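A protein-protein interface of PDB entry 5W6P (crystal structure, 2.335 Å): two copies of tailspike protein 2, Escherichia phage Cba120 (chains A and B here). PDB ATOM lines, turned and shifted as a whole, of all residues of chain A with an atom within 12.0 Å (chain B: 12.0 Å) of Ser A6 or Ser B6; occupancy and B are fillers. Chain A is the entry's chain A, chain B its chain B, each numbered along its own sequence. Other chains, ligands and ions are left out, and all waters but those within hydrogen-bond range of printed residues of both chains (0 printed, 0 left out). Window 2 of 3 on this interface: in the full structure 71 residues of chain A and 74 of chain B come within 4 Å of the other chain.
Of the 13 printed residues of chain B, 5 touch a printed residue of chain A. Hydrophobic or aromatic side chains of chain B that line the printed part of chain A: Phe B7, Val B10 and Leu B14. Of the 13 printed residues of chain A, 6 touch a printed residue of chain B. Hydrophobic or aromatic side chains of chain A that line the printed part of chain B: Val A10 and Leu A14. Among the printed residues, 8 pairs touch across the chains. Among the printed residues, no Asp or Glu carboxylate lies within 4 Å of a Lys or Arg side-chain nitrogen of the other chain.
The backbone carbonyl oxygen (O) of Asp A5 sits close to the side-chain amide oxygen (OD1) of Asn A9, at 3.3 Å. The backbone carbonyl oxygen (O) of Asn A9 lies within hydrogen-bond range of the side-chain hydroxyl (OG1) of Thr A13.
The backbone carbonyl oxygen (O) of Tyr A22 lies close to the backbone carbonyl oxygen (O) of Leu B14 (3.1 Å).
Ser B6 touches its own counterpart, Ser A6. Val A10 touches its own counterpart, Val B10. Leu B14 touches its own counterpart, Leu A14. Tyr A22 touches Leu B14, but with the chains exchanged Leu A14 does not touch Tyr B22 (8.1 Å). Of the 8 pairs that touch across the chains among the printed residues, 3 have their exchanged pair printed and touching as well.
No residue of chain B comes within 4 Å of Asp A5. Of chain B, only Ser B6 comes within 4 Å of Ser A6. No residue of chain B comes within 4 Å of Ile A8. Printed residues of chain B within 4 Å of Val A10: Phe B7 (3.5 Å) and Val B10 (3.6 Å). Of the printed residues of chain B, Leu A14 touches Leu B14 (3.8 Å). Of the printed residues of chain B, Tyr A22 touches Leu B14 (3.1 Å) and Gly B15 (3.6 Å). No residue of chain A comes within 4 Å of Asp B5. Of chain A, only Ser A6 (3.8 Å) comes within 4 Å of Ser B6. Ile B11 touches none of the printed residues of chain A. Printed residues of chain A within 4 Å of Leu B14: Leu A14 and Tyr A22. Of the printed residues of chain A, Gly B15 touches Tyr A22. The nearest residue of chain B that does not touch Ser A6 is Phe B7 (4.2 Å). The nearest residue of chain A that does not touch Ser B6 is Val A10 (5.1 Å).
OG of Ser A6 touches CB of Ser B6 (3.8 Å). O of Asn A9 touches CE1 of Phe B7 (3.8 Å). CG2 of Val A10 touches CD1 of Phe B7, 3.5 Å away. Val A10 touches Val B10 (CG2 to CG1, 3.6 Å). OG1 of Thr A13 touches CE1 of Phe B7, at 3.5 Å. Leu B14 touches Leu A14 (CD1 to CD2, 3.8 Å). N of Gly B15 touches O of Tyr A22, 3.6 Å away.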
ATOM      1  N   ASP A   5       1.168  -0.788 -27.311  1.00  0.00           N
ATOM      2  CA  ASP A   5       2.316   0.111 -27.280  1.00  0.00           C
ATOM      3  C   ASP A   5       3.613  -0.650 -27.029  1.00  0.00           C
ATOM      4  O   ASP A   5       4.626  -0.398 -27.684  1.00  0.00           O
ATOM      5  CB  ASP A   5       2.129   1.190 -26.218  1.00  0.00           C
ATOM      6  CG  ASP A   5       3.157   2.297 -26.330  1.00  0.00           C
ATOM      7  OD1 ASP A   5       3.140   3.017 -27.349  1.00  0.00           O
ATOM      8  OD2 ASP A   5       3.981   2.445 -25.401  1.00  0.00           O
ATOM      9  N   SER A   6       3.583  -1.589 -26.080  1.00  0.00           N
ATOM     10  CA  SER A   6       4.774  -2.395 -25.840  1.00  0.00           C
ATOM     11  C   SER A   6       5.063  -3.259 -27.057  1.00  0.00           C
ATOM     12  O   SER A   6       6.224  -3.572 -27.342  1.00  0.00           O
ATOM     13  CB  SER A   6       4.599  -3.245 -24.580  1.00  0.00           C
ATOM     14  OG  SER A   6       3.565  -4.203 -24.742  1.00  0.00           O
ATOM     15  N   PHE A   7       4.007  -3.640 -27.777  1.00  0.00           N
ATOM     16  CA  PHE A   7       4.159  -4.295 -29.068  1.00  0.00           C
ATOM     17  C   PHE A   7       5.015  -3.453 -30.007  1.00  0.00           C
ATOM     18  O   PHE A   7       5.956  -3.955 -30.634  1.00  0.00           O
ATOM     19  CB  PHE A   7       2.774  -4.536 -29.678  1.00  0.00           C
ATOM     20  CG  PHE A   7       2.792  -5.261 -31.001  1.00  0.00           C
ATOM     21  CD1 PHE A   7       2.911  -4.552 -32.187  1.00  0.00           C
ATOM     22  CD2 PHE A   7       2.662  -6.639 -31.062  1.00  0.00           C
ATOM     23  CE1 PHE A   7       2.919  -5.201 -33.406  1.00  0.00           C
ATOM     24  CE2 PHE A   7       2.668  -7.295 -32.279  1.00  0.00           C
ATOM     25  CZ  PHE A   7       2.797  -6.572 -33.452  1.00  0.00           C
ATOM     26  N   ILE A   8       4.699  -2.161 -30.112  1.00  0.00           N
ATOM     27  CA  ILE A   8       5.376  -1.314 -31.086  1.00  0.00           C
ATOM     28  C   ILE A   8       6.845  -1.099 -30.726  1.00  0.00           C
ATOM     29  O   ILE A   8       7.701  -1.040 -31.619  1.00  0.00           O
ATOM     30  CB  ILE A   8       4.609   0.012 -31.230  1.00  0.00           C
ATOM     31  CG1 ILE A   8       3.212  -0.263 -31.799  1.00  0.00           C
ATOM     32  CG2 ILE A   8       5.363   0.973 -32.132  1.00  0.00           C
ATOM     33  CD1 ILE A   8       2.162   0.746 -31.397  1.00  0.00           C
ATOM     34  N   ASN A   9       7.182  -1.016 -29.434  1.00  0.00           N
ATOM     35  CA  ASN A   9       8.593  -0.876 -29.079  1.00  0.00           C
ATOM     36  C   ASN A   9       9.370  -2.151 -29.360  1.00  0.00           C
ATOM     37  O   ASN A   9      10.524  -2.092 -29.803  1.00  0.00           O
ATOM     38  CB  ASN A   9       8.767  -0.450 -27.623  1.00  0.00           C
ATOM     39  CG  ASN A   9       8.461   1.013 -27.409  1.00  0.00           C
ATOM     40  OD1 ASN A   9       7.304   1.411 -27.278  1.00  0.00           O
ATOM     41  ND2 ASN A   9       9.512   1.832 -27.377  1.00  0.00           N
ATOM     42  N   VAL A  10       8.768  -3.313 -29.105  1.00  0.00           N
ATOM     43  CA  VAL A  10       9.444  -4.563 -29.439  1.00  0.00           C
ATOM     44  C   VAL A  10       9.692  -4.637 -30.939  1.00  0.00           C
ATOM     45  O   VAL A  10      10.814  -4.895 -31.388  1.00  0.00           O
ATOM     46  CB  VAL A  10       8.629  -5.775 -28.949  1.00  0.00           C
ATOM     47  CG1 VAL A  10       9.113  -7.044 -29.637  1.00  0.00           C
ATOM     48  CG2 VAL A  10       8.733  -5.917 -27.439  1.00  0.00           C
ATOM     49  N   ILE A  11       8.655  -4.372 -31.736  1.00  0.00           N
ATOM     50  CA  ILE A  11       8.783  -4.477 -33.186  1.00  0.00           C
ATOM     51  C   ILE A  11       9.828  -3.497 -33.701  1.00  0.00           C
ATOM     52  O   ILE A  11      10.662  -3.840 -34.550  1.00  0.00           O
ATOM     53  CB  ILE A  11       7.416  -4.242 -33.855  1.00  0.00           C
ATOM     54  CG1 ILE A  11       6.500  -5.447 -33.642  1.00  0.00           C
ATOM     55  CG2 ILE A  11       7.592  -3.993 -35.340  1.00  0.00           C
ATOM     56  CD1 ILE A  11       7.110  -6.763 -34.040  1.00  0.00           C
ATOM     57  N   ASN A  12       9.811  -2.266 -33.186  1.00  0.00           N
ATOM     58  CA  ASN A  12      10.781  -1.261 -33.605  1.00  0.00           C
ATOM     59  C   ASN A  12      12.196  -1.644 -33.189  1.00  0.00           C
ATOM     60  O   ASN A  12      13.157  -1.382 -33.923  1.00  0.00           O
ATOM     61  CB  ASN A  12      10.401   0.101 -33.027  1.00  0.00           C
ATOM     62  CG  ASN A  12       9.335   0.801 -33.842  1.00  0.00           C
ATOM     63  OD1 ASN A  12       9.166   0.535 -35.031  1.00  0.00           O
ATOM     64  ND2 ASN A  12       8.603   1.698 -33.201  1.00  0.00           N
ATOM     65  N   THR A  13      12.346  -2.265 -32.017  1.00  0.00           N
ATOM     66  CA  THR A  13      13.676  -2.631 -31.537  1.00  0.00           C
ATOM     67  C   THR A  13      14.308  -3.703 -32.424  1.00  0.00           C
ATOM     68  O   THR A  13      15.482  -3.599 -32.796  1.00  0.00           O
ATOM     69  CB  THR A  13      13.597  -3.099 -30.083  1.00  0.00           C
ATOM     70  OG1 THR A  13      13.180  -2.005 -29.254  1.00  0.00           O
ATOM     71  CG2 THR A  13      14.956  -3.586 -29.611  1.00  0.00           C
ATOM     72  N   LEU A  14      13.560  -4.757 -32.752  1.00  0.00           N
ATOM     73  CA  LEU A  14      14.086  -5.758 -33.670  1.00  0.00           C
ATOM     74  C   LEU A  14      14.319  -5.205 -35.072  1.00  0.00           C
ATOM     75  O   LEU A  14      15.140  -5.758 -35.810  1.00  0.00           O
ATOM     76  CB  LEU A  14      13.171  -6.990 -33.727  1.00  0.00           C
ATOM     77  CG  LEU A  14      13.106  -7.906 -32.493  1.00  0.00           C
ATOM     78  CD1 LEU A  14      13.413  -7.171 -31.209  1.00  0.00           C
ATOM     79  CD2 LEU A  14      11.778  -8.655 -32.403  1.00  0.00           C
ATOM     80  N   GLY A  15      13.633  -4.135 -35.455  1.00  0.00           N
ATOM     81  CA  GLY A  15      13.788  -3.621 -36.800  1.00  0.00           C
ATOM     82  C   GLY A  15      15.005  -2.751 -37.059  1.00  0.00           C
ATOM     83  O   GLY A  15      15.218  -2.355 -38.206  1.00  0.00           O
ATOM     84  N   ARG A  16      15.794  -2.417 -36.042  1.00  0.00           N
ATOM     85  CA  ARG A  16      17.017  -1.661 -36.269  1.00  0.00           C
ATOM     86  C   ARG A  16      18.060  -2.508 -36.998  1.00  0.00           C
ATOM     87  O   ARG A  16      17.960  -3.735 -37.078  1.00  0.00           O
ATOM     88  CB  ARG A  16      17.576  -1.129 -34.953  1.00  0.00           C
ATOM     89  CG  ARG A  16      16.719  -0.040 -34.353  1.00  0.00           C
ATOM     90  CD  ARG A  16      17.325   0.509 -33.082  1.00  0.00           C
ATOM     91  NE  ARG A  16      16.707   1.774 -32.701  1.00  0.00           N
ATOM     92  CZ  ARG A  16      15.726   1.886 -31.807  1.00  0.00           C
ATOM     93  NH1 ARG A  16      15.226   3.085 -31.513  1.00  0.00           N
ATOM     94  NH2 ARG A  16      15.221   0.805 -31.225  1.00  0.00           N
ATOM     95  N   TYR A  22      19.211  -9.413 -30.864  1.00  0.00           N
ATOM     96  CA  TYR A  22      18.218  -9.741 -29.844  1.00  0.00           C
ATOM     97  C   TYR A  22      17.727 -11.178 -29.923  1.00  0.00           C
ATOM     98  O   TYR A  22      17.057 -11.637 -28.990  1.00  0.00           O
ATOM     99  CB  TYR A  22      17.016  -8.801 -29.929  1.00  0.00           C
ATOM    100  CG  TYR A  22      17.385  -7.378 -29.640  1.00  0.00           C
ATOM    101  CD1 TYR A  22      17.683  -6.971 -28.347  1.00  0.00           C
ATOM    102  CD2 TYR A  22      17.459  -6.443 -30.660  1.00  0.00           C
ATOM    103  CE1 TYR A  22      18.036  -5.667 -28.076  1.00  0.00           C
ATOM    104  CE2 TYR A  22      17.806  -5.137 -30.398  1.00  0.00           C
ATOM    105  CZ  TYR A  22      18.096  -4.754 -29.109  1.00  0.00           C
ATOM    106  OH  TYR A  22      18.446  -3.452 -28.861  1.00  0.00           O
ATOM    107  N   ASP B   5       7.329  -3.098 -18.966  1.00  0.00           N
ATOM    108  CA  ASP B   5       6.728  -4.312 -18.426  1.00  0.00           C
ATOM    109  C   ASP B   5       6.877  -5.503 -19.382  1.00  0.00           C
ATOM    110  O   ASP B   5       7.796  -6.307 -19.242  1.00  0.00           O
ATOM    111  CB  ASP B   5       5.244  -4.070 -18.097  1.00  0.00           C
ATOM    112  CG  ASP B   5       4.452  -3.522 -19.281  1.00  0.00           C
ATOM    113  OD1 ASP B   5       5.078  -3.184 -20.311  1.00  0.00           O
ATOM    114  OD2 ASP B   5       3.208  -3.451 -19.195  1.00  0.00           O
ATOM    115  N   SER B   6       5.973  -5.589 -20.363  1.00  0.00           N
ATOM    116  CA  SER B   6       6.013  -6.674 -21.333  1.00  0.00           C
ATOM    117  C   SER B   6       7.212  -6.552 -22.259  1.00  0.00           C
ATOM    118  O   SER B   6       7.756  -7.570 -22.701  1.00  0.00           O
ATOM    119  CB  SER B   6       4.721  -6.701 -22.148  1.00  0.00           C
ATOM    120  OG  SER B   6       3.589  -6.805 -21.302  1.00  0.00           O
ATOM    121  N   PHE B   7       7.641  -5.325 -22.558  1.00  0.00           N
ATOM    122  CA  PHE B   7       8.833  -5.142 -23.375  1.00  0.00           C
ATOM    123  C   PHE B   7      10.046  -5.854 -22.795  1.00  0.00           C
ATOM    124  O   PHE B   7      10.706  -6.640 -23.487  1.00  0.00           O
ATOM    125  CB  PHE B   7       9.150  -3.661 -23.540  1.00  0.00           C
ATOM    126  CG  PHE B   7      10.404  -3.420 -24.314  1.00  0.00           C
ATOM    127  CD1 PHE B   7      10.412  -3.451 -25.696  1.00  0.00           C
ATOM    128  CD2 PHE B   7      11.604  -3.217 -23.643  1.00  0.00           C
ATOM    129  CE1 PHE B   7      11.594  -3.249 -26.398  1.00  0.00           C
ATOM    130  CE2 PHE B   7      12.787  -3.020 -24.335  1.00  0.00           C
ATOM    131  CZ  PHE B   7      12.783  -3.033 -25.713  1.00  0.00           C
ATOM    132  N   ILE B   8      10.353  -5.613 -21.519  1.00  0.00           N
ATOM    133  CA  ILE B   8      11.590  -6.177 -20.996  1.00  0.00           C
ATOM    134  C   ILE B   8      11.493  -7.694 -20.980  1.00  0.00           C
ATOM    135  O   ILE B   8      12.486  -8.395 -21.215  1.00  0.00           O
ATOM    136  CB  ILE B   8      11.891  -5.643 -19.584  1.00  0.00           C
ATOM    137  CG1 ILE B   8      12.045  -4.125 -19.586  1.00  0.00           C
ATOM    138  CG2 ILE B   8      13.172  -6.263 -19.052  1.00  0.00           C
ATOM    139  CD1 ILE B   8      10.716  -3.391 -19.490  1.00  0.00           C
ATOM    140  N   ASN B   9      10.288  -8.218 -20.740  1.00  0.00           N
ATOM    141  CA  ASN B   9      10.076  -9.659 -20.707  1.00  0.00           C
ATOM    142  C   ASN B   9      10.176 -10.279 -22.096  1.00  0.00           C
ATOM    143  O   ASN B   9      10.754 -11.360 -22.260  1.00  0.00           O
ATOM    144  CB  ASN B   9       8.715  -9.947 -20.086  1.00  0.00           C
ATOM    145  CG  ASN B   9       8.666  -9.567 -18.624  1.00  0.00           C
ATOM    146  OD1 ASN B   9       9.671  -9.651 -17.919  1.00  0.00           O
ATOM    147  ND2 ASN B   9       7.500  -9.123 -18.162  1.00  0.00           N
ATOM    148  N   VAL B  10       9.632  -9.604 -23.109  1.00  0.00           N
ATOM    149  CA  VAL B  10       9.732 -10.107 -24.476  1.00  0.00           C
ATOM    150  C   VAL B  10      11.194 -10.221 -24.885  1.00  0.00           C
ATOM    151  O   VAL B  10      11.625 -11.236 -25.444  1.00  0.00           O
ATOM    152  CB  VAL B  10       8.944  -9.202 -25.441  1.00  0.00           C
ATOM    153  CG1 VAL B  10       9.374  -9.460 -26.877  1.00  0.00           C
ATOM    154  CG2 VAL B  10       7.454  -9.443 -25.291  1.00  0.00           C
ATOM    155  N   ILE B  11      11.978  -9.180 -24.608  1.00  0.00           N
ATOM    156  CA  ILE B  11      13.383  -9.172 -25.000  1.00  0.00           C
ATOM    157  C   ILE B  11      14.139 -10.322 -24.341  1.00  0.00           C
ATOM    158  O   ILE B  11      14.943 -11.006 -24.988  1.00  0.00           O
ATOM    159  CB  ILE B  11      14.008  -7.808 -24.659  1.00  0.00           C
ATOM    160  CG1 ILE B  11      13.524  -6.741 -25.644  1.00  0.00           C
ATOM    161  CG2 ILE B  11      15.523  -7.898 -24.652  1.00  0.00           C
ATOM    162  CD1 ILE B  11      13.710  -7.107 -27.097  1.00  0.00           C
ATOM    163  N   ASN B  12      13.893 -10.560 -23.051  1.00  0.00           N
ATOM    164  CA  ASN B  12      14.571 -11.656 -22.361  1.00  0.00           C
ATOM    165  C   ASN B  12      14.171 -13.019 -22.914  1.00  0.00           C
ATOM    166  O   ASN B  12      14.999 -13.938 -22.943  1.00  0.00           O
ATOM    167  CB  ASN B  12      14.325 -11.572 -20.857  1.00  0.00           C
ATOM    168  CG  ASN B  12      15.298 -10.632 -20.166  1.00  0.00           C
ATOM    169  OD1 ASN B  12      16.405 -10.396 -20.659  1.00  0.00           O
ATOM    170  ND2 ASN B  12      14.887 -10.074 -19.030  1.00  0.00           N
ATOM    171  N   THR B  13      12.914 -13.184 -23.331  1.00  0.00           N
ATOM    172  CA  THR B  13      12.501 -14.454 -23.922  1.00  0.00           C
ATOM    173  C   THR B  13      13.223 -14.686 -25.243  1.00  0.00           C
ATOM    174  O   THR B  13      13.744 -15.779 -25.496  1.00  0.00           O
ATOM    175  CB  THR B  13      10.990 -14.475 -24.139  1.00  0.00           C
ATOM    176  OG1 THR B  13      10.326 -14.448 -22.873  1.00  0.00           O
ATOM    177  CG2 THR B  13      10.574 -15.719 -24.904  1.00  0.00           C
ATOM    178  N   LEU B  14      13.249 -13.666 -26.104  1.00  0.00           N
ATOM    179  CA  LEU B  14      13.965 -13.759 -27.372  1.00  0.00           C
ATOM    180  C   LEU B  14      15.466 -13.910 -27.167  1.00  0.00           C
ATOM    181  O   LEU B  14      16.154 -14.468 -28.028  1.00  0.00           O
ATOM    182  CB  LEU B  14      13.679 -12.518 -28.221  1.00  0.00           C
ATOM    183  CG  LEU B  14      12.231 -12.286 -28.657  1.00  0.00           C
ATOM    184  CD1 LEU B  14      12.122 -11.017 -29.472  1.00  0.00           C
ATOM    185  CD2 LEU B  14      11.729 -13.471 -29.465  1.00  0.00           C
ATOM    186  N   GLY B  15      15.992 -13.427 -26.044  1.00  0.00           N
ATOM    187  CA  GLY B  15      17.425 -13.496 -25.838  1.00  0.00           C
ATOM    188  C   GLY B  15      17.950 -14.808 -25.303  1.00  0.00           C
ATOM    189  O   GLY B  15      19.170 -14.974 -25.226  1.00  0.00           O
ATOM    190  N   ARG B  16      17.076 -15.746 -24.939  1.00  0.00           N
ATOM    191  CA  ARG B  16      17.548 -17.040 -24.469  1.00  0.00           C
ATOM    192  C   ARG B  16      18.160 -17.847 -25.612  1.00  0.00           C
ATOM    193  O   ARG B  16      18.021 -17.523 -26.796  1.00  0.00           O
ATOM    194  CB  ARG B  16      16.434 -17.816 -23.763  1.00  0.00           C
ATOM    195  CG  ARG B  16      16.008 -17.181 -22.439  1.00  0.00           C
ATOM    196  CD  ARG B  16      15.037 -18.070 -21.664  1.00  0.00           C
ATOM    197  NE  ARG B  16      14.942 -17.649 -20.267  1.00  0.00           N
ATOM    198  CZ  ARG B  16      13.947 -16.931 -19.751  1.00  0.00           C
ATOM    199  NH1 ARG B  16      12.927 -16.559 -20.511  1.00  0.00           N
ATOM    200  NH2 ARG B  16      13.962 -16.607 -18.465  1.00  0.00           N
ATOM    201  N   TYR B  22      11.349 -18.451 -32.147  1.00  0.00           N
ATOM    202  CA  TYR B  22      10.216 -17.536 -32.218  1.00  0.00           C
ATOM    203  C   TYR B  22      10.061 -16.838 -33.565  1.00  0.00           C
ATOM    204  O   TYR B  22       9.040 -16.182 -33.787  1.00  0.00           O
ATOM    205  CB  TYR B  22      10.319 -16.486 -31.106  1.00  0.00           C
ATOM    206  CG  TYR B  22      10.304 -17.090 -29.716  1.00  0.00           C
ATOM    207  CD1 TYR B  22       9.141 -17.629 -29.177  1.00  0.00           C
ATOM    208  CD2 TYR B  22      11.457 -17.119 -28.944  1.00  0.00           C
ATOM    209  CE1 TYR B  22       9.135 -18.183 -27.909  1.00  0.00           C
ATOM    210  CE2 TYR B  22      11.458 -17.670 -27.678  1.00  0.00           C
ATOM    211  CZ  TYR B  22      10.300 -18.201 -27.168  1.00  0.00           C
ATOM    212  OH  TYR B  22      10.314 -18.741 -25.905  1.00  0.00           O
